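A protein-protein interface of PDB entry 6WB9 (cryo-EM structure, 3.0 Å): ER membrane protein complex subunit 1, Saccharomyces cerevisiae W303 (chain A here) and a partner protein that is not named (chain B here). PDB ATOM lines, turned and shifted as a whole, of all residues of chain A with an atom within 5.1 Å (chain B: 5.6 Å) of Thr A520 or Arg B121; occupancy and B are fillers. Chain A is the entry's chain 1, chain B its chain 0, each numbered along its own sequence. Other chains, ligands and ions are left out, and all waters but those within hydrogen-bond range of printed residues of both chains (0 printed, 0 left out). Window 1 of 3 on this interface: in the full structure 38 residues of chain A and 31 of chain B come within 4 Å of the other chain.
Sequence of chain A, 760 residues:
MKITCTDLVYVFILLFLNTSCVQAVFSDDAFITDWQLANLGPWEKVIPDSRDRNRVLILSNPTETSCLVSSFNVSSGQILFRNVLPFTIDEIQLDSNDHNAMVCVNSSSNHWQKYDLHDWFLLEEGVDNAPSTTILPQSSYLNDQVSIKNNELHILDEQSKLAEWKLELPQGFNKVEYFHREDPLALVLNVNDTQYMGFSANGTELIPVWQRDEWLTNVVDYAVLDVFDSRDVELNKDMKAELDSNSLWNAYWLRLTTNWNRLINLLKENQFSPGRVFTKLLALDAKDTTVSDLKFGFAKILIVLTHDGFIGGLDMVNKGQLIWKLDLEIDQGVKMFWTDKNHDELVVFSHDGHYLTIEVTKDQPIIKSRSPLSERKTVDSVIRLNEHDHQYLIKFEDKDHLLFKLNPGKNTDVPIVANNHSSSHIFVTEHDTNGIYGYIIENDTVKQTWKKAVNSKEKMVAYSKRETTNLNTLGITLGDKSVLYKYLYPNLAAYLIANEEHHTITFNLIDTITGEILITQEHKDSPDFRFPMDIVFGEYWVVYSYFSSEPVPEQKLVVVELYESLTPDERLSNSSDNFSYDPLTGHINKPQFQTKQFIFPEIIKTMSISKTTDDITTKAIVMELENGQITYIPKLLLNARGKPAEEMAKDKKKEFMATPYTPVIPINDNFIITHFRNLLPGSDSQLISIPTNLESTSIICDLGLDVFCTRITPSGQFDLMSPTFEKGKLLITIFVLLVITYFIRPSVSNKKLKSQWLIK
N of Glu B124 lies within hydrogen-bond range of O of Thr A520, at 3.3 Å.
O of Glu B124 lies within hydrogen-bond range of N of Glu A522 (2.7 Å).
NH2 of Arg B121 lies within hydrogen-bond range of O of Leu A518 (3.3 Å).
The guanidinium group of Arg B121 lies within hydrogen-bond range of the backbone carbonyl oxygen of Ile A517, 2.5 Å away.
O of Ser B106 is in hydrogen-bond range of N of Ile B93.
O of Gln A521 sits at hydrogen-bond distance from N of Phe A507 (2.9 Å).
The backbone NH (N) of Val B96 is in hydrogen-bond range of the backbone carbonyl oxygen (O) of Arg B121, 3.0 Å away.
The side-chain hydroxyl of Thr A506 lies within hydrogen-bond range of the side-chain carboxylate of Glu A522, at 2.4 Å.
The side-chain carboxylate (OD1) of Asp B95 is in salt-bridge range of the guanidinium group (NE) of Arg B121, at 2.5 Å.
N of Arg B121 is in hydrogen-bond range of O of Val B94, at 2.9 Å.
Among the printed residues, merely in contact across the chains: Ile A517 with Ser B106 (3.9 Å), Thr A520 with Arg B121 (3.9 Å), Thr A520 with Pro B123 (3.2 Å), Gln A521 with Glu B124 (3.3 Å), Glu A522 with Pro B123 (3.6 Å) and Phe A593 with Glu B124 (3.5 Å).
Thr A520 touches just these residues of chain B: Arg B121 (3.9 Å), Pro B123 (3.2 Å) and Glu B124 (3.3 Å).
Arg B121 touches just these residues of chain A: Ile A517, Leu A518 and Thr A520.
Of the printed residues of chain B, Ile A517 touches Ser B106 and Arg B121.
Printed residues of chain B within 4 Å of Leu A518: Arg B121.
Thr B119 touches none of the printed residues of chain A.
The nearest residue of chain A that does not touch Arg B121 is Ile A519 (4.7 Å).
The nearest printed residue of chain B that does not touch Ile A517 is Asp B95 (4.2 Å).
Printed residues of chain B that touch a printed residue of chain A: Ser B106, Arg B121, Pro B123 and Glu B124.
Printed residues of chain A that touch a printed residue of chain B: Ile A517, Leu A518, Thr A520, Gln A521, Glu A522 and Phe A593.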
ATOM      1  N   THR A 506       2.116 -23.302 -19.499  1.00  0.00           N
ATOM      2  CA  THR A 506       0.698 -23.615 -19.419  1.00  0.00           C
ATOM      3  C   THR A 506       0.536 -24.952 -18.711  1.00  0.00           C
ATOM      4  O   THR A 506       0.768 -26.008 -19.303  1.00  0.00           O
ATOM      5  CB  THR A 506       0.078 -23.650 -20.811  1.00  0.00           C
ATOM      6  OG1 THR A 506       0.518 -22.509 -21.557  1.00  0.00           O
ATOM      7  CG2 THR A 506      -1.420 -23.615 -20.713  1.00  0.00           C
ATOM      8  N   PHE A 507       0.164 -24.901 -17.440  1.00  0.00           N
ATOM      9  CA  PHE A 507      -0.205 -26.097 -16.702  1.00  0.00           C
ATOM     10  C   PHE A 507      -1.599 -26.531 -17.127  1.00  0.00           C
ATOM     11  O   PHE A 507      -2.542 -25.740 -17.055  1.00  0.00           O
ATOM     12  CB  PHE A 507      -0.154 -25.825 -15.202  1.00  0.00           C
ATOM     13  CG  PHE A 507      -0.936 -26.802 -14.382  1.00  0.00           C
ATOM     14  CD1 PHE A 507      -0.475 -28.088 -14.195  1.00  0.00           C
ATOM     15  CD2 PHE A 507      -2.125 -26.429 -13.781  1.00  0.00           C
ATOM     16  CE1 PHE A 507      -1.191 -28.983 -13.442  1.00  0.00           C
ATOM     17  CE2 PHE A 507      -2.843 -27.326 -13.029  1.00  0.00           C
ATOM     18  CZ  PHE A 507      -2.375 -28.602 -12.859  1.00  0.00           C
ATOM     19  N   ASN A 508      -1.736 -27.775 -17.572  1.00  0.00           N
ATOM     20  CA  ASN A 508      -3.026 -28.321 -17.951  1.00  0.00           C
ATOM     21  C   ASN A 508      -3.304 -29.593 -17.169  1.00  0.00           C
ATOM     22  O   ASN A 508      -2.393 -30.360 -16.848  1.00  0.00           O
ATOM     23  CB  ASN A 508      -3.095 -28.622 -19.446  1.00  0.00           C
ATOM     24  CG  ASN A 508      -2.889 -27.398 -20.302  1.00  0.00           C
ATOM     25  OD1 ASN A 508      -3.847 -26.758 -20.725  1.00  0.00           O
ATOM     26  ND2 ASN A 508      -1.636 -27.073 -20.576  1.00  0.00           N
ATOM     27  N   ILE A 517      -9.648 -30.780 -20.848  1.00  0.00           N
ATOM     28  CA  ILE A 517      -8.721 -30.051 -19.991  1.00  0.00           C
ATOM     29  C   ILE A 517      -9.522 -29.417 -18.861  1.00  0.00           C
ATOM     30  O   ILE A 517     -10.279 -28.469 -19.078  1.00  0.00           O
ATOM     31  CB  ILE A 517      -7.938 -29.000 -20.777  1.00  0.00           C
ATOM     32  CG1 ILE A 517      -7.197 -29.664 -21.935  1.00  0.00           C
ATOM     33  CG2 ILE A 517      -6.963 -28.287 -19.868  1.00  0.00           C
ATOM     34  CD1 ILE A 517      -6.409 -28.706 -22.778  1.00  0.00           C
ATOM     35  N   LEU A 518      -9.350 -29.938 -17.646  1.00  0.00           N
ATOM     36  CA  LEU A 518     -10.141 -29.474 -16.515  1.00  0.00           C
ATOM     37  C   LEU A 518      -9.634 -28.145 -15.972  1.00  0.00           C
ATOM     38  O   LEU A 518     -10.433 -27.268 -15.627  1.00  0.00           O
ATOM     39  CB  LEU A 518     -10.137 -30.525 -15.409  1.00  0.00           C
ATOM     40  CG  LEU A 518     -10.641 -31.915 -15.778  1.00  0.00           C
ATOM     41  CD1 LEU A 518     -10.675 -32.789 -14.554  1.00  0.00           C
ATOM     42  CD2 LEU A 518     -12.012 -31.836 -16.401  1.00  0.00           C
ATOM     43  N   ILE A 519      -8.318 -27.980 -15.877  1.00  0.00           N
ATOM     44  CA  ILE A 519      -7.702 -26.817 -15.249  1.00  0.00           C
ATOM     45  C   ILE A 519      -6.571 -26.342 -16.147  1.00  0.00           C
ATOM     46  O   ILE A 519      -5.744 -27.146 -16.584  1.00  0.00           O
ATOM     47  CB  ILE A 519      -7.185 -27.148 -13.833  1.00  0.00           C
ATOM     48  CG1 ILE A 519      -8.351 -27.317 -12.862  1.00  0.00           C
ATOM     49  CG2 ILE A 519      -6.243 -26.081 -13.311  1.00  0.00           C
ATOM     50  CD1 ILE A 519      -7.945 -27.843 -11.542  1.00  0.00           C
ATOM     51  N   THR A 520      -6.547 -25.044 -16.438  1.00  0.00           N
ATOM     52  CA  THR A 520      -5.487 -24.421 -17.211  1.00  0.00           C
ATOM     53  C   THR A 520      -4.885 -23.282 -16.400  1.00  0.00           C
ATOM     54  O   THR A 520      -5.598 -22.586 -15.674  1.00  0.00           O
ATOM     55  CB  THR A 520      -6.025 -23.899 -18.541  1.00  0.00           C
ATOM     56  OG1 THR A 520      -6.545 -24.996 -19.298  1.00  0.00           O
ATOM     57  CG2 THR A 520      -4.926 -23.248 -19.338  1.00  0.00           C
ATOM     58  N   GLN A 521      -3.573 -23.098 -16.515  1.00  0.00           N
ATOM     59  CA  GLN A 521      -2.859 -22.087 -15.739  1.00  0.00           C
ATOM     60  C   GLN A 521      -1.726 -21.516 -16.574  1.00  0.00           C
ATOM     61  O   GLN A 521      -0.796 -22.242 -16.925  1.00  0.00           O
ATOM     62  CB  GLN A 521      -2.310 -22.670 -14.445  1.00  0.00           C
ATOM     63  CG  GLN A 521      -3.224 -22.538 -13.273  1.00  0.00           C
ATOM     64  CD  GLN A 521      -2.471 -22.191 -12.025  1.00  0.00           C
ATOM     65  OE1 GLN A 521      -1.454 -22.805 -11.709  1.00  0.00           O
ATOM     66  NE2 GLN A 521      -2.949 -21.186 -11.312  1.00  0.00           N
ATOM     67  N   GLU A 522      -1.785 -20.224 -16.874  1.00  0.00           N
ATOM     68  CA  GLU A 522      -0.698 -19.562 -17.577  1.00  0.00           C
ATOM     69  C   GLU A 522       0.261 -18.903 -16.601  1.00  0.00           C
ATOM     70  O   GLU A 522      -0.155 -18.256 -15.637  1.00  0.00           O
ATOM     71  CB  GLU A 522      -1.222 -18.510 -18.550  1.00  0.00           C
ATOM     72  CG  GLU A 522      -1.678 -19.058 -19.877  1.00  0.00           C
ATOM     73  CD  GLU A 522      -0.557 -19.314 -20.855  1.00  0.00           C
ATOM     74  OE1 GLU A 522       0.188 -20.296 -20.669  1.00  0.00           O
ATOM     75  OE2 GLU A 522      -0.434 -18.539 -21.826  1.00  0.00           O
ATOM     76  N   PHE A 593      -9.561 -25.562  -7.712  1.00  0.00           N
ATOM     77  CA  PHE A 593      -8.168 -25.640  -7.316  1.00  0.00           C
ATOM     78  C   PHE A 593      -7.762 -24.443  -6.471  1.00  0.00           C
ATOM     79  O   PHE A 593      -8.397 -23.387  -6.483  1.00  0.00           O
ATOM     80  CB  PHE A 593      -7.254 -25.755  -8.544  1.00  0.00           C
ATOM     81  CG  PHE A 593      -7.299 -24.567  -9.471  1.00  0.00           C
ATOM     82  CD1 PHE A 593      -8.294 -24.443 -10.427  1.00  0.00           C
ATOM     83  CD2 PHE A 593      -6.318 -23.598  -9.414  1.00  0.00           C
ATOM     84  CE1 PHE A 593      -8.323 -23.365 -11.280  1.00  0.00           C
ATOM     85  CE2 PHE A 593      -6.339 -22.519 -10.264  1.00  0.00           C
ATOM     86  CZ  PHE A 593      -7.342 -22.402 -11.197  1.00  0.00           C
ATOM     87  N   ILE B  93     -16.039 -26.047 -24.364  1.00  0.00           N
ATOM     88  CA  ILE B  93     -15.062 -25.136 -23.789  1.00  0.00           C
ATOM     89  C   ILE B  93     -13.981 -24.881 -24.828  1.00  0.00           C
ATOM     90  O   ILE B  93     -13.279 -25.804 -25.251  1.00  0.00           O
ATOM     91  CB  ILE B  93     -14.470 -25.709 -22.495  1.00  0.00           C
ATOM     92  CG1 ILE B  93     -15.538 -25.730 -21.402  1.00  0.00           C
ATOM     93  CG2 ILE B  93     -13.271 -24.904 -22.065  1.00  0.00           C
ATOM     94  CD1 ILE B  93     -15.040 -26.214 -20.068  1.00  0.00           C
ATOM     95  N   VAL B  94     -13.862 -23.632 -25.256  1.00  0.00           N
ATOM     96  CA  VAL B  94     -12.866 -23.223 -26.236  1.00  0.00           C
ATOM     97  C   VAL B  94     -11.764 -22.511 -25.460  1.00  0.00           C
ATOM     98  O   VAL B  94     -11.895 -21.340 -25.106  1.00  0.00           O
ATOM     99  CB  VAL B  94     -13.476 -22.330 -27.320  1.00  0.00           C
ATOM    100  CG1 VAL B  94     -12.428 -21.930 -28.334  1.00  0.00           C
ATOM    101  CG2 VAL B  94     -14.625 -23.045 -28.002  1.00  0.00           C
ATOM    102  N   ASP B  95     -10.692 -23.235 -25.147  1.00  0.00           N
ATOM    103  CA  ASP B  95      -9.558 -22.649 -24.448  1.00  0.00           C
ATOM    104  C   ASP B  95      -8.768 -21.780 -25.414  1.00  0.00           C
ATOM    105  O   ASP B  95      -8.216 -22.286 -26.399  1.00  0.00           O
ATOM    106  CB  ASP B  95      -8.669 -23.745 -23.869  1.00  0.00           C
ATOM    107  CG  ASP B  95      -9.298 -24.444 -22.684  1.00  0.00           C
ATOM    108  OD1 ASP B  95      -9.560 -23.769 -21.669  1.00  0.00           O
ATOM    109  OD2 ASP B  95      -9.536 -25.666 -22.769  1.00  0.00           O
ATOM    110  N   VAL B  96      -8.684 -20.484 -25.102  1.00  0.00           N
ATOM    111  CA  VAL B  96      -8.086 -19.501 -26.003  1.00  0.00           C
ATOM    112  C   VAL B  96      -6.769 -19.000 -25.427  1.00  0.00           C
ATOM    113  O   VAL B  96      -6.334 -19.450 -24.364  1.00  0.00           O
ATOM    114  CB  VAL B  96      -9.041 -18.325 -26.271  1.00  0.00           C
ATOM    115  CG1 VAL B  96     -10.272 -18.801 -27.018  1.00  0.00           C
ATOM    116  CG2 VAL B  96      -9.424 -17.656 -24.972  1.00  0.00           C
ATOM    117  N   SER B 106     -12.390 -28.494 -25.826  1.00  0.00           N
ATOM    118  CA  SER B 106     -12.773 -29.648 -25.029  1.00  0.00           C
ATOM    119  C   SER B 106     -14.280 -29.619 -24.831  1.00  0.00           C
ATOM    120  O   SER B 106     -14.935 -28.605 -25.066  1.00  0.00           O
ATOM    121  CB  SER B 106     -12.042 -29.678 -23.680  1.00  0.00           C
ATOM    122  OG  SER B 106     -12.165 -28.445 -22.997  1.00  0.00           O
ATOM    123  N   THR B 119     -18.613 -21.982 -24.666  1.00  0.00           N
ATOM    124  CA  THR B 119     -18.049 -20.952 -23.807  1.00  0.00           C
ATOM    125  C   THR B 119     -16.555 -20.865 -24.063  1.00  0.00           C
ATOM    126  O   THR B 119     -15.870 -21.890 -24.107  1.00  0.00           O
ATOM    127  CB  THR B 119     -18.299 -21.249 -22.326  1.00  0.00           C
ATOM    128  OG1 THR B 119     -17.649 -22.474 -21.968  1.00  0.00           O
ATOM    129  CG2 THR B 119     -19.783 -21.372 -22.041  1.00  0.00           C
ATOM    130  N   VAL B 120     -16.054 -19.648 -24.237  1.00  0.00           N
ATOM    131  CA  VAL B 120     -14.617 -19.427 -24.319  1.00  0.00           C
ATOM    132  C   VAL B 120     -14.051 -19.435 -22.905  1.00  0.00           C
ATOM    133  O   VAL B 120     -14.613 -18.819 -21.991  1.00  0.00           O
ATOM    134  CB  VAL B 120     -14.308 -18.116 -25.067  1.00  0.00           C
ATOM    135  CG1 VAL B 120     -12.818 -17.775 -25.074  1.00  0.00           C
ATOM    136  CG2 VAL B 120     -14.797 -18.211 -26.493  1.00  0.00           C
ATOM    137  N   ARG B 121     -12.972 -20.183 -22.711  1.00  0.00           N
ATOM    138  CA  ARG B 121     -12.249 -20.198 -21.452  1.00  0.00           C
ATOM    139  C   ARG B 121     -10.895 -19.544 -21.669  1.00  0.00           C
ATOM    140  O   ARG B 121     -10.109 -19.983 -22.520  1.00  0.00           O
ATOM    141  CB  ARG B 121     -12.086 -21.618 -20.918  1.00  0.00           C
ATOM    142  CG  ARG B 121     -11.502 -21.684 -19.522  1.00  0.00           C
ATOM    143  CD  ARG B 121     -11.664 -23.064 -18.919  1.00  0.00           C
ATOM    144  NE  ARG B 121     -10.903 -24.076 -19.643  1.00  0.00           N
ATOM    145  CZ  ARG B 121     -10.931 -25.373 -19.360  1.00  0.00           C
ATOM    146  NH1 ARG B 121     -10.209 -26.222 -20.073  1.00  0.00           N
ATOM    147  NH2 ARG B 121     -11.689 -25.820 -18.371  1.00  0.00           N
ATOM    148  N   TYR B 122     -10.650 -18.480 -20.928  1.00  0.00           N
ATOM    149  CA  TYR B 122      -9.301 -17.961 -20.830  1.00  0.00           C
ATOM    150  C   TYR B 122      -8.558 -18.705 -19.728  1.00  0.00           C
ATOM    151  O   TYR B 122      -9.143 -19.007 -18.684  1.00  0.00           O
ATOM    152  CB  TYR B 122      -9.312 -16.467 -20.533  1.00  0.00           C
ATOM    153  CG  TYR B 122      -9.438 -15.618 -21.771  1.00  0.00           C
ATOM    154  CD1 TYR B 122      -8.308 -15.198 -22.458  1.00  0.00           C
ATOM    155  CD2 TYR B 122     -10.683 -15.248 -22.261  1.00  0.00           C
ATOM    156  CE1 TYR B 122      -8.413 -14.424 -23.596  1.00  0.00           C
ATOM    157  CE2 TYR B 122     -10.798 -14.474 -23.399  1.00  0.00           C
ATOM    158  CZ  TYR B 122      -9.659 -14.067 -24.061  1.00  0.00           C
ATOM    159  OH  TYR B 122      -9.762 -13.296 -25.194  1.00  0.00           O
ATOM    160  N   PRO B 123      -7.294 -19.038 -19.968  1.00  0.00           N
ATOM    161  CA  PRO B 123      -6.519 -19.769 -18.961  1.00  0.00           C
ATOM    162  C   PRO B 123      -6.255 -18.904 -17.744  1.00  0.00           C
ATOM    163  O   PRO B 123      -6.061 -17.691 -17.855  1.00  0.00           O
ATOM    164  CB  PRO B 123      -5.222 -20.114 -19.696  1.00  0.00           C
ATOM    165  CG  PRO B 123      -5.145 -19.118 -20.794  1.00  0.00           C
ATOM    166  CD  PRO B 123      -6.526 -18.805 -21.198  1.00  0.00           C
ATOM    167  N   GLU B 124      -6.291 -19.539 -16.577  1.00  0.00           N
ATOM    168  CA  GLU B 124      -6.141 -18.823 -15.323  1.00  0.00           C
ATOM    169  C   GLU B 124      -4.732 -18.272 -15.196  1.00  0.00           C
ATOM    170  O   GLU B 124      -3.763 -18.895 -15.633  1.00  0.00           O
ATOM    171  CB  GLU B 124      -6.444 -19.747 -14.146  1.00  0.00           C
ATOM    172  CG  GLU B 124      -7.782 -20.442 -14.237  1.00  0.00           C
ATOM    173  CD  GLU B 124      -8.770 -19.935 -13.210  1.00  0.00           C
ATOM    174  OE1 GLU B 124      -8.350 -19.194 -12.297  1.00  0.00           O
ATOM    175  OE2 GLU B 124      -9.967 -20.275 -13.314  1.00  0.00           O
